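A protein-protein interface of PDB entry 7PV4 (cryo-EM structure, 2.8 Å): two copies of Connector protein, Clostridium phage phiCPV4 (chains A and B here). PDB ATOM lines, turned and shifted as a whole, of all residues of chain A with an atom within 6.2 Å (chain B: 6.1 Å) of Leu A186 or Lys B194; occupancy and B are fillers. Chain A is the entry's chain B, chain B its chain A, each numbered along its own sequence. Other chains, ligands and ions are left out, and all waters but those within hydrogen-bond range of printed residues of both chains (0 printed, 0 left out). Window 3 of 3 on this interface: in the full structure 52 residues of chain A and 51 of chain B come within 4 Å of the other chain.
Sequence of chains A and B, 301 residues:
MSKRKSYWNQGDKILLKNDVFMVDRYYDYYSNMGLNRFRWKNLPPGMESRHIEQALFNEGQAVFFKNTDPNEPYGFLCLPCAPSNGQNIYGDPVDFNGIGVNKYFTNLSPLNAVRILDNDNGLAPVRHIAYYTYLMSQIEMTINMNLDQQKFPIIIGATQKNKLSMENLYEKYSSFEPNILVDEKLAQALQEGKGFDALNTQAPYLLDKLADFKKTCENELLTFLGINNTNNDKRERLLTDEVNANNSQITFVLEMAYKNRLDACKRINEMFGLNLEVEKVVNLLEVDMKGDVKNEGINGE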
ATOM      1  N   GLY A 157      30.439 -21.398  27.497  1.00  0.00           N
ATOM      2  CA  GLY A 157      29.808 -22.609  28.013  1.00  0.00           C
ATOM      3  C   GLY A 157      30.745 -23.808  27.896  1.00  0.00           C
ATOM      4  O   GLY A 157      31.403 -23.990  26.884  1.00  0.00           O
ATOM      5  N   ALA A 158      30.859 -24.629  28.930  1.00  0.00           N
ATOM      6  CA  ALA A 158      31.748 -25.792  28.938  1.00  0.00           C
ATOM      7  C   ALA A 158      31.156 -26.983  29.708  1.00  0.00           C
ATOM      8  O   ALA A 158      30.132 -26.853  30.377  1.00  0.00           O
ATOM      9  CB  ALA A 158      33.108 -25.374  29.494  1.00  0.00           C
ATOM     10  N   THR A 159      31.783 -28.155  29.619  1.00  0.00           N
ATOM     11  CA  THR A 159      31.534 -29.246  30.576  1.00  0.00           C
ATOM     12  C   THR A 159      32.127 -28.894  31.940  1.00  0.00           C
ATOM     13  O   THR A 159      33.003 -28.041  32.051  1.00  0.00           O
ATOM     14  CB  THR A 159      32.097 -30.594  30.109  1.00  0.00           C
ATOM     15  OG1 THR A 159      33.465 -30.642  30.375  1.00  0.00           O
ATOM     16  CG2 THR A 159      31.885 -30.887  28.635  1.00  0.00           C
ATOM     17  N   ASP A 183      27.340 -25.650  30.835  1.00  0.00           N
ATOM     18  CA  ASP A 183      26.131 -25.855  30.044  1.00  0.00           C
ATOM     19  C   ASP A 183      25.652 -27.305  30.224  1.00  0.00           C
ATOM     20  O   ASP A 183      26.346 -28.255  29.874  1.00  0.00           O
ATOM     21  CB  ASP A 183      26.425 -25.452  28.596  1.00  0.00           C
ATOM     22  CG  ASP A 183      25.243 -25.646  27.627  1.00  0.00           C
ATOM     23  OD1 ASP A 183      24.348 -26.472  27.889  1.00  0.00           O
ATOM     24  OD2 ASP A 183      25.211 -24.949  26.592  1.00  0.00           O
ATOM     25  N   GLU A 184      24.451 -27.476  30.772  1.00  0.00           N
ATOM     26  CA  GLU A 184      23.849 -28.784  31.008  1.00  0.00           C
ATOM     27  C   GLU A 184      23.582 -29.589  29.723  1.00  0.00           C
ATOM     28  O   GLU A 184      23.827 -30.790  29.717  1.00  0.00           O
ATOM     29  CB  GLU A 184      22.594 -28.635  31.868  1.00  0.00           C
ATOM     30  CG  GLU A 184      21.403 -27.980  31.158  1.00  0.00           C
ATOM     31  CD  GLU A 184      20.249 -27.692  32.123  1.00  0.00           C
ATOM     32  OE1 GLU A 184      19.891 -28.563  32.934  1.00  0.00           O
ATOM     33  OE2 GLU A 184      19.675 -26.591  32.066  1.00  0.00           O
ATOM     34  N   LYS A 185      23.168 -28.978  28.607  1.00  0.00           N
ATOM     35  CA  LYS A 185      23.050 -29.702  27.334  1.00  0.00           C
ATOM     36  C   LYS A 185      24.425 -30.142  26.849  1.00  0.00           C
ATOM     37  O   LYS A 185      24.594 -31.286  26.446  1.00  0.00           O
ATOM     38  CB  LYS A 185      22.364 -28.855  26.252  1.00  0.00           C
ATOM     39  CG  LYS A 185      20.861 -28.621  26.425  1.00  0.00           C
ATOM     40  CD  LYS A 185      20.054 -29.927  26.406  1.00  0.00           C
ATOM     41  CE  LYS A 185      18.575 -29.704  26.077  1.00  0.00           C
ATOM     42  NZ  LYS A 185      17.892 -28.862  27.086  1.00  0.00           N
ATOM     43  N   LEU A 186      25.424 -29.270  26.934  1.00  0.00           N
ATOM     44  CA  LEU A 186      26.782 -29.586  26.481  1.00  0.00           C
ATOM     45  C   LEU A 186      27.390 -30.742  27.280  1.00  0.00           C
ATOM     46  O   LEU A 186      27.960 -31.665  26.713  1.00  0.00           O
ATOM     47  CB  LEU A 186      27.634 -28.315  26.572  1.00  0.00           C
ATOM     48  CG  LEU A 186      28.817 -28.290  25.606  1.00  0.00           C
ATOM     49  CD1 LEU A 186      28.364 -27.953  24.186  1.00  0.00           C
ATOM     50  CD2 LEU A 186      29.807 -27.238  26.084  1.00  0.00           C
ATOM     51  N   ALA A 187      27.233 -30.712  28.604  1.00  0.00           N
ATOM     52  CA  ALA A 187      27.652 -31.775  29.504  1.00  0.00           C
ATOM     53  C   ALA A 187      26.871 -33.091  29.319  1.00  0.00           C
ATOM     54  O   ALA A 187      27.461 -34.160  29.430  1.00  0.00           O
ATOM     55  CB  ALA A 187      27.519 -31.248  30.937  1.00  0.00           C
ATOM     56  N   GLN A 188      25.560 -33.044  29.057  1.00  0.00           N
ATOM     57  CA  GLN A 188      24.710 -34.237  28.899  1.00  0.00           C
ATOM     58  C   GLN A 188      25.001 -35.012  27.620  1.00  0.00           C
ATOM     59  O   GLN A 188      25.191 -36.223  27.660  1.00  0.00           O
ATOM     60  CB  GLN A 188      23.225 -33.847  28.870  1.00  0.00           C
ATOM     61  CG  GLN A 188      22.633 -33.523  30.249  1.00  0.00           C
ATOM     62  CD  GLN A 188      21.338 -32.710  30.175  1.00  0.00           C
ATOM     63  OE1 GLN A 188      20.984 -31.979  31.082  1.00  0.00           O
ATOM     64  NE2 GLN A 188      20.558 -32.803  29.122  1.00  0.00           N
ATOM     65  N   ALA A 189      24.957 -34.343  26.472  1.00  0.00           N
ATOM     66  CA  ALA A 189      24.885 -34.996  25.170  1.00  0.00           C
ATOM     67  C   ALA A 189      26.116 -35.847  24.828  1.00  0.00           C
ATOM     68  O   ALA A 189      27.262 -35.434  25.025  1.00  0.00           O
ATOM     69  CB  ALA A 189      24.610 -33.939  24.099  1.00  0.00           C
ATOM     70  N   GLY A 193      29.296 -31.976  19.298  1.00  0.00           N
ATOM     71  CA  GLY A 193      29.282 -30.867  20.263  1.00  0.00           C
ATOM     72  C   GLY A 193      30.603 -30.780  21.020  1.00  0.00           C
ATOM     73  O   GLY A 193      31.093 -31.787  21.528  1.00  0.00           O
ATOM     74  N   LYS A 194      31.220 -29.595  21.033  1.00  0.00           N
ATOM     75  CA  LYS A 194      32.668 -29.441  21.253  1.00  0.00           C
ATOM     76  C   LYS A 194      33.156 -29.546  22.699  1.00  0.00           C
ATOM     77  O   LYS A 194      34.337 -29.755  22.883  1.00  0.00           O
ATOM     78  CB  LYS A 194      33.154 -28.112  20.628  1.00  0.00           C
ATOM     79  CG  LYS A 194      33.854 -28.230  19.265  1.00  0.00           C
ATOM     80  CD  LYS A 194      34.987 -29.260  19.059  1.00  0.00           C
ATOM     81  CE  LYS A 194      35.809 -29.735  20.266  1.00  0.00           C
ATOM     82  NZ  LYS A 194      36.357 -28.641  21.095  1.00  0.00           N
ATOM     83  N   GLY A 195      32.334 -29.344  23.720  1.00  0.00           N
ATOM     84  CA  GLY A 195      32.805 -29.278  25.124  1.00  0.00           C
ATOM     85  C   GLY A 195      33.328 -27.912  25.599  1.00  0.00           C
ATOM     86  O   GLY A 195      33.529 -27.722  26.794  1.00  0.00           O
ATOM     87  N   PHE A 196      33.479 -26.959  24.685  1.00  0.00           N
ATOM     88  CA  PHE A 196      33.554 -25.518  24.892  1.00  0.00           C
ATOM     89  C   PHE A 196      32.730 -24.851  23.792  1.00  0.00           C
ATOM     90  O   PHE A 196      32.909 -25.206  22.634  1.00  0.00           O
ATOM     91  CB  PHE A 196      35.002 -25.015  24.795  1.00  0.00           C
ATOM     92  CG  PHE A 196      35.930 -25.406  25.922  1.00  0.00           C
ATOM     93  CD1 PHE A 196      35.868 -24.716  27.143  1.00  0.00           C
ATOM     94  CD2 PHE A 196      36.902 -26.398  25.731  1.00  0.00           C
ATOM     95  CE1 PHE A 196      36.779 -25.011  28.167  1.00  0.00           C
ATOM     96  CE2 PHE A 196      37.808 -26.701  26.757  1.00  0.00           C
ATOM     97  CZ  PHE A 196      37.754 -25.998  27.969  1.00  0.00           C
ATOM     98  N   ASP A 197      31.878 -23.877  24.090  1.00  0.00           N
ATOM     99  CA  ASP A 197      31.289 -23.000  23.078  1.00  0.00           C
ATOM    100  C   ASP A 197      31.149 -21.548  23.562  1.00  0.00           C
ATOM    101  O   ASP A 197      30.690 -21.258  24.656  1.00  0.00           O
ATOM    102  CB  ASP A 197      29.989 -23.563  22.481  1.00  0.00           C
ATOM    103  CG  ASP A 197      28.763 -23.757  23.393  1.00  0.00           C
ATOM    104  OD1 ASP A 197      28.859 -23.755  24.627  1.00  0.00           O
ATOM    105  OD2 ASP A 197      27.663 -23.927  22.828  1.00  0.00           O
ATOM    106  N   ASN B 162      20.520 -23.513  33.272  1.00  0.00           N
ATOM    107  CA  ASN B 162      21.467 -22.614  32.635  1.00  0.00           C
ATOM    108  C   ASN B 162      21.223 -21.157  33.038  1.00  0.00           C
ATOM    109  O   ASN B 162      22.188 -20.486  33.397  1.00  0.00           O
ATOM    110  CB  ASN B 162      21.429 -22.822  31.116  1.00  0.00           C
ATOM    111  CG  ASN B 162      22.245 -24.012  30.639  1.00  0.00           C
ATOM    112  OD1 ASN B 162      22.792 -24.789  31.400  1.00  0.00           O
ATOM    113  ND2 ASN B 162      22.385 -24.159  29.351  1.00  0.00           N
ATOM    114  N   LEU B 186      13.507 -24.512  23.975  1.00  0.00           N
ATOM    115  CA  LEU B 186      14.895 -24.875  24.272  1.00  0.00           C
ATOM    116  C   LEU B 186      14.984 -25.849  25.451  1.00  0.00           C
ATOM    117  O   LEU B 186      15.687 -26.848  25.389  1.00  0.00           O
ATOM    118  CB  LEU B 186      15.692 -23.591  24.528  1.00  0.00           C
ATOM    119  CG  LEU B 186      17.186 -23.719  24.241  1.00  0.00           C
ATOM    120  CD1 LEU B 186      17.467 -23.663  22.740  1.00  0.00           C
ATOM    121  CD2 LEU B 186      17.910 -22.575  24.934  1.00  0.00           C
ATOM    122  N   GLU B 192      19.623 -32.160  19.544  1.00  0.00           N
ATOM    123  CA  GLU B 192      20.283 -30.894  19.177  1.00  0.00           C
ATOM    124  C   GLU B 192      19.536 -29.604  19.581  1.00  0.00           C
ATOM    125  O   GLU B 192      18.333 -29.587  19.845  1.00  0.00           O
ATOM    126  CB  GLU B 192      20.605 -30.896  17.669  1.00  0.00           C
ATOM    127  CG  GLU B 192      22.021 -31.411  17.379  1.00  0.00           C
ATOM    128  CD  GLU B 192      23.141 -30.480  17.886  1.00  0.00           C
ATOM    129  OE1 GLU B 192      22.850 -29.459  18.548  1.00  0.00           O
ATOM    130  OE2 GLU B 192      24.325 -30.768  17.618  1.00  0.00           O
ATOM    131  N   GLY B 193      20.284 -28.503  19.644  1.00  0.00           N
ATOM    132  CA  GLY B 193      19.899 -27.234  20.280  1.00  0.00           C
ATOM    133  C   GLY B 193      20.722 -26.978  21.539  1.00  0.00           C
ATOM    134  O   GLY B 193      20.851 -27.862  22.383  1.00  0.00           O
ATOM    135  N   LYS B 194      21.341 -25.797  21.632  1.00  0.00           N
ATOM    136  CA  LYS B 194      22.529 -25.573  22.472  1.00  0.00           C
ATOM    137  C   LYS B 194      22.282 -25.396  23.972  1.00  0.00           C
ATOM    138  O   LYS B 194      23.226 -25.540  24.720  1.00  0.00           O
ATOM    139  CB  LYS B 194      23.338 -24.373  21.926  1.00  0.00           C
ATOM    140  CG  LYS B 194      24.579 -24.726  21.093  1.00  0.00           C
ATOM    141  CD  LYS B 194      25.607 -25.751  21.625  1.00  0.00           C
ATOM    142  CE  LYS B 194      25.741 -25.975  23.139  1.00  0.00           C
ATOM    143  NZ  LYS B 194      25.915 -24.733  23.923  1.00  0.00           N
ATOM    144  N   GLY B 195      21.097 -25.026  24.437  1.00  0.00           N
ATOM    145  CA  GLY B 195      20.865 -24.690  25.862  1.00  0.00           C
ATOM    146  C   GLY B 195      21.200 -23.248  26.279  1.00  0.00           C
ATOM    147  O   GLY B 195      20.837 -22.835  27.375  1.00  0.00           O
ATOM    148  N   PHE B 196      21.822 -22.478  25.392  1.00  0.00           N
ATOM    149  CA  PHE B 196      21.889 -21.022  25.355  1.00  0.00           C
ATOM    150  C   PHE B 196      21.716 -20.591  23.899  1.00  0.00           C
ATOM    151  O   PHE B 196      22.387 -21.150  23.042  1.00  0.00           O
ATOM    152  CB  PHE B 196      23.248 -20.514  25.860  1.00  0.00           C
ATOM    153  CG  PHE B 196      23.518 -20.667  27.339  1.00  0.00           C
ATOM    154  CD1 PHE B 196      22.944 -19.764  28.246  1.00  0.00           C
ATOM    155  CD2 PHE B 196      24.399 -21.655  27.801  1.00  0.00           C
ATOM    156  CE1 PHE B 196      23.255 -19.843  29.612  1.00  0.00           C
ATOM    157  CE2 PHE B 196      24.703 -21.743  29.168  1.00  0.00           C
ATOM    158  CZ  PHE B 196      24.142 -20.827  30.069  1.00  0.00           C
ATOM    159  N   ASP B 197      20.892 -19.597  23.588  1.00  0.00           N
ATOM    160  CA  ASP B 197      20.899 -18.938  22.282  1.00  0.00           C
ATOM    161  C   ASP B 197      20.650 -17.425  22.382  1.00  0.00           C
ATOM    162  O   ASP B 197      19.756 -16.947  23.064  1.00  0.00           O
ATOM    163  CB  ASP B 197      19.989 -19.631  21.255  1.00  0.00           C
ATOM    164  CG  ASP B 197      18.471 -19.680  21.506  1.00  0.00           C
ATOM    165  OD1 ASP B 197      17.983 -19.446  22.620  1.00  0.00           O
ATOM    166  OD2 ASP B 197      17.749 -19.977  20.532  1.00  0.00           O
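Printed residues of chain B within 4 Å of Asp A183: Asn B162, Lys B194 and Phe B196.
Of the printed residues of chain B, Lys A185 touches Leu B186, Lys B194 and Gly B195.
Of chain B, only Lys B194 comes within 4 Å of Leu A186.
Ala A187 touches none of the printed residues of chain B.
Ala A189 touches none of the printed residues of chain B.
Of the printed residues of chain A, Leu B186 touches Lys A185 (3.4 Å).
Printed residues of chain A within 4 Å of Gly B195: Lys A185.
Printed residues of chain A within 4 Å of Phe B196: Asp A183.
Among the printed residues, merely in contact across the chains: Leu A186 with Lys B194, Asp A183 with Phe B196, Lys A185 with Lys B194 and Lys A185 with Gly B195.
Of the 8 printed residues of chain B, 5 touch a printed residue of chain A.
Among the printed residues, 9 pairs touch across the chains.
Among the printed residues, Asp or Glu carboxylates within 4 Å of a Lys or Arg side-chain nitrogen of the other chain: Asp A183 with Lys B194 and Asp A197 with Lys B194.
The backbone NH (N) of Asp A197 sits at hydrogen-bond distance from the backbone carbonyl oxygen (O) of Gly A157 (2.8 Å).
O of Glu A184 sits close to OE1 of Gln A188 (3.4 Å).
The backbone NH of Lys A185 is in hydrogen-bond range of the side-chain carboxylate of Asp A183, 2.9 Å away.
OD1 of Asp A183 lies within hydrogen-bond range of N of Leu A186, 3.1 Å away.
The side-chain amide nitrogen of Asn B162 is in hydrogen-bond range of the backbone carbonyl oxygen of Gly B195, 2.8 Å away.
The backbone NH (N) of Asp A183 is in hydrogen-bond range of the backbone carbonyl oxygen (O) of Ala A158 (3.1 Å).
OD1 of Asp A183 sits at hydrogen-bond distance from ND2 of Asn B162, at 3.4 Å.
NZ of Lys B194 lies within salt-bridge range of OD2 of Asp A183 (2.8 Å).
The backbone carbonyl oxygen (O) of Leu B186 is in hydrogen-bond range of the side-chain amino group (NZ) of Lys A185, 3.4 Å away.
The side-chain amino group (NZ) of Lys B194 lies within salt-bridge range of the side-chain carboxylate (OD1) of Asp A197, 3.2 Å away.
The backbone NH (N) of Glu A184 sits at hydrogen-bond distance from the side-chain amide oxygen (OD1) of Asn B162, 3.2 Å away.
Leu A186 touches Lys B194, but with the chains exchanged Lys A194 does not touch Leu B186 (15.1 Å).
Asp A197 touches Lys B194, but with the chains exchanged Lys A194 does not touch Asp B197 (14.6 Å).
Of the 9 pairs that touch across the chains among the printed residues, none has its exchanged pair printed and touching as well.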
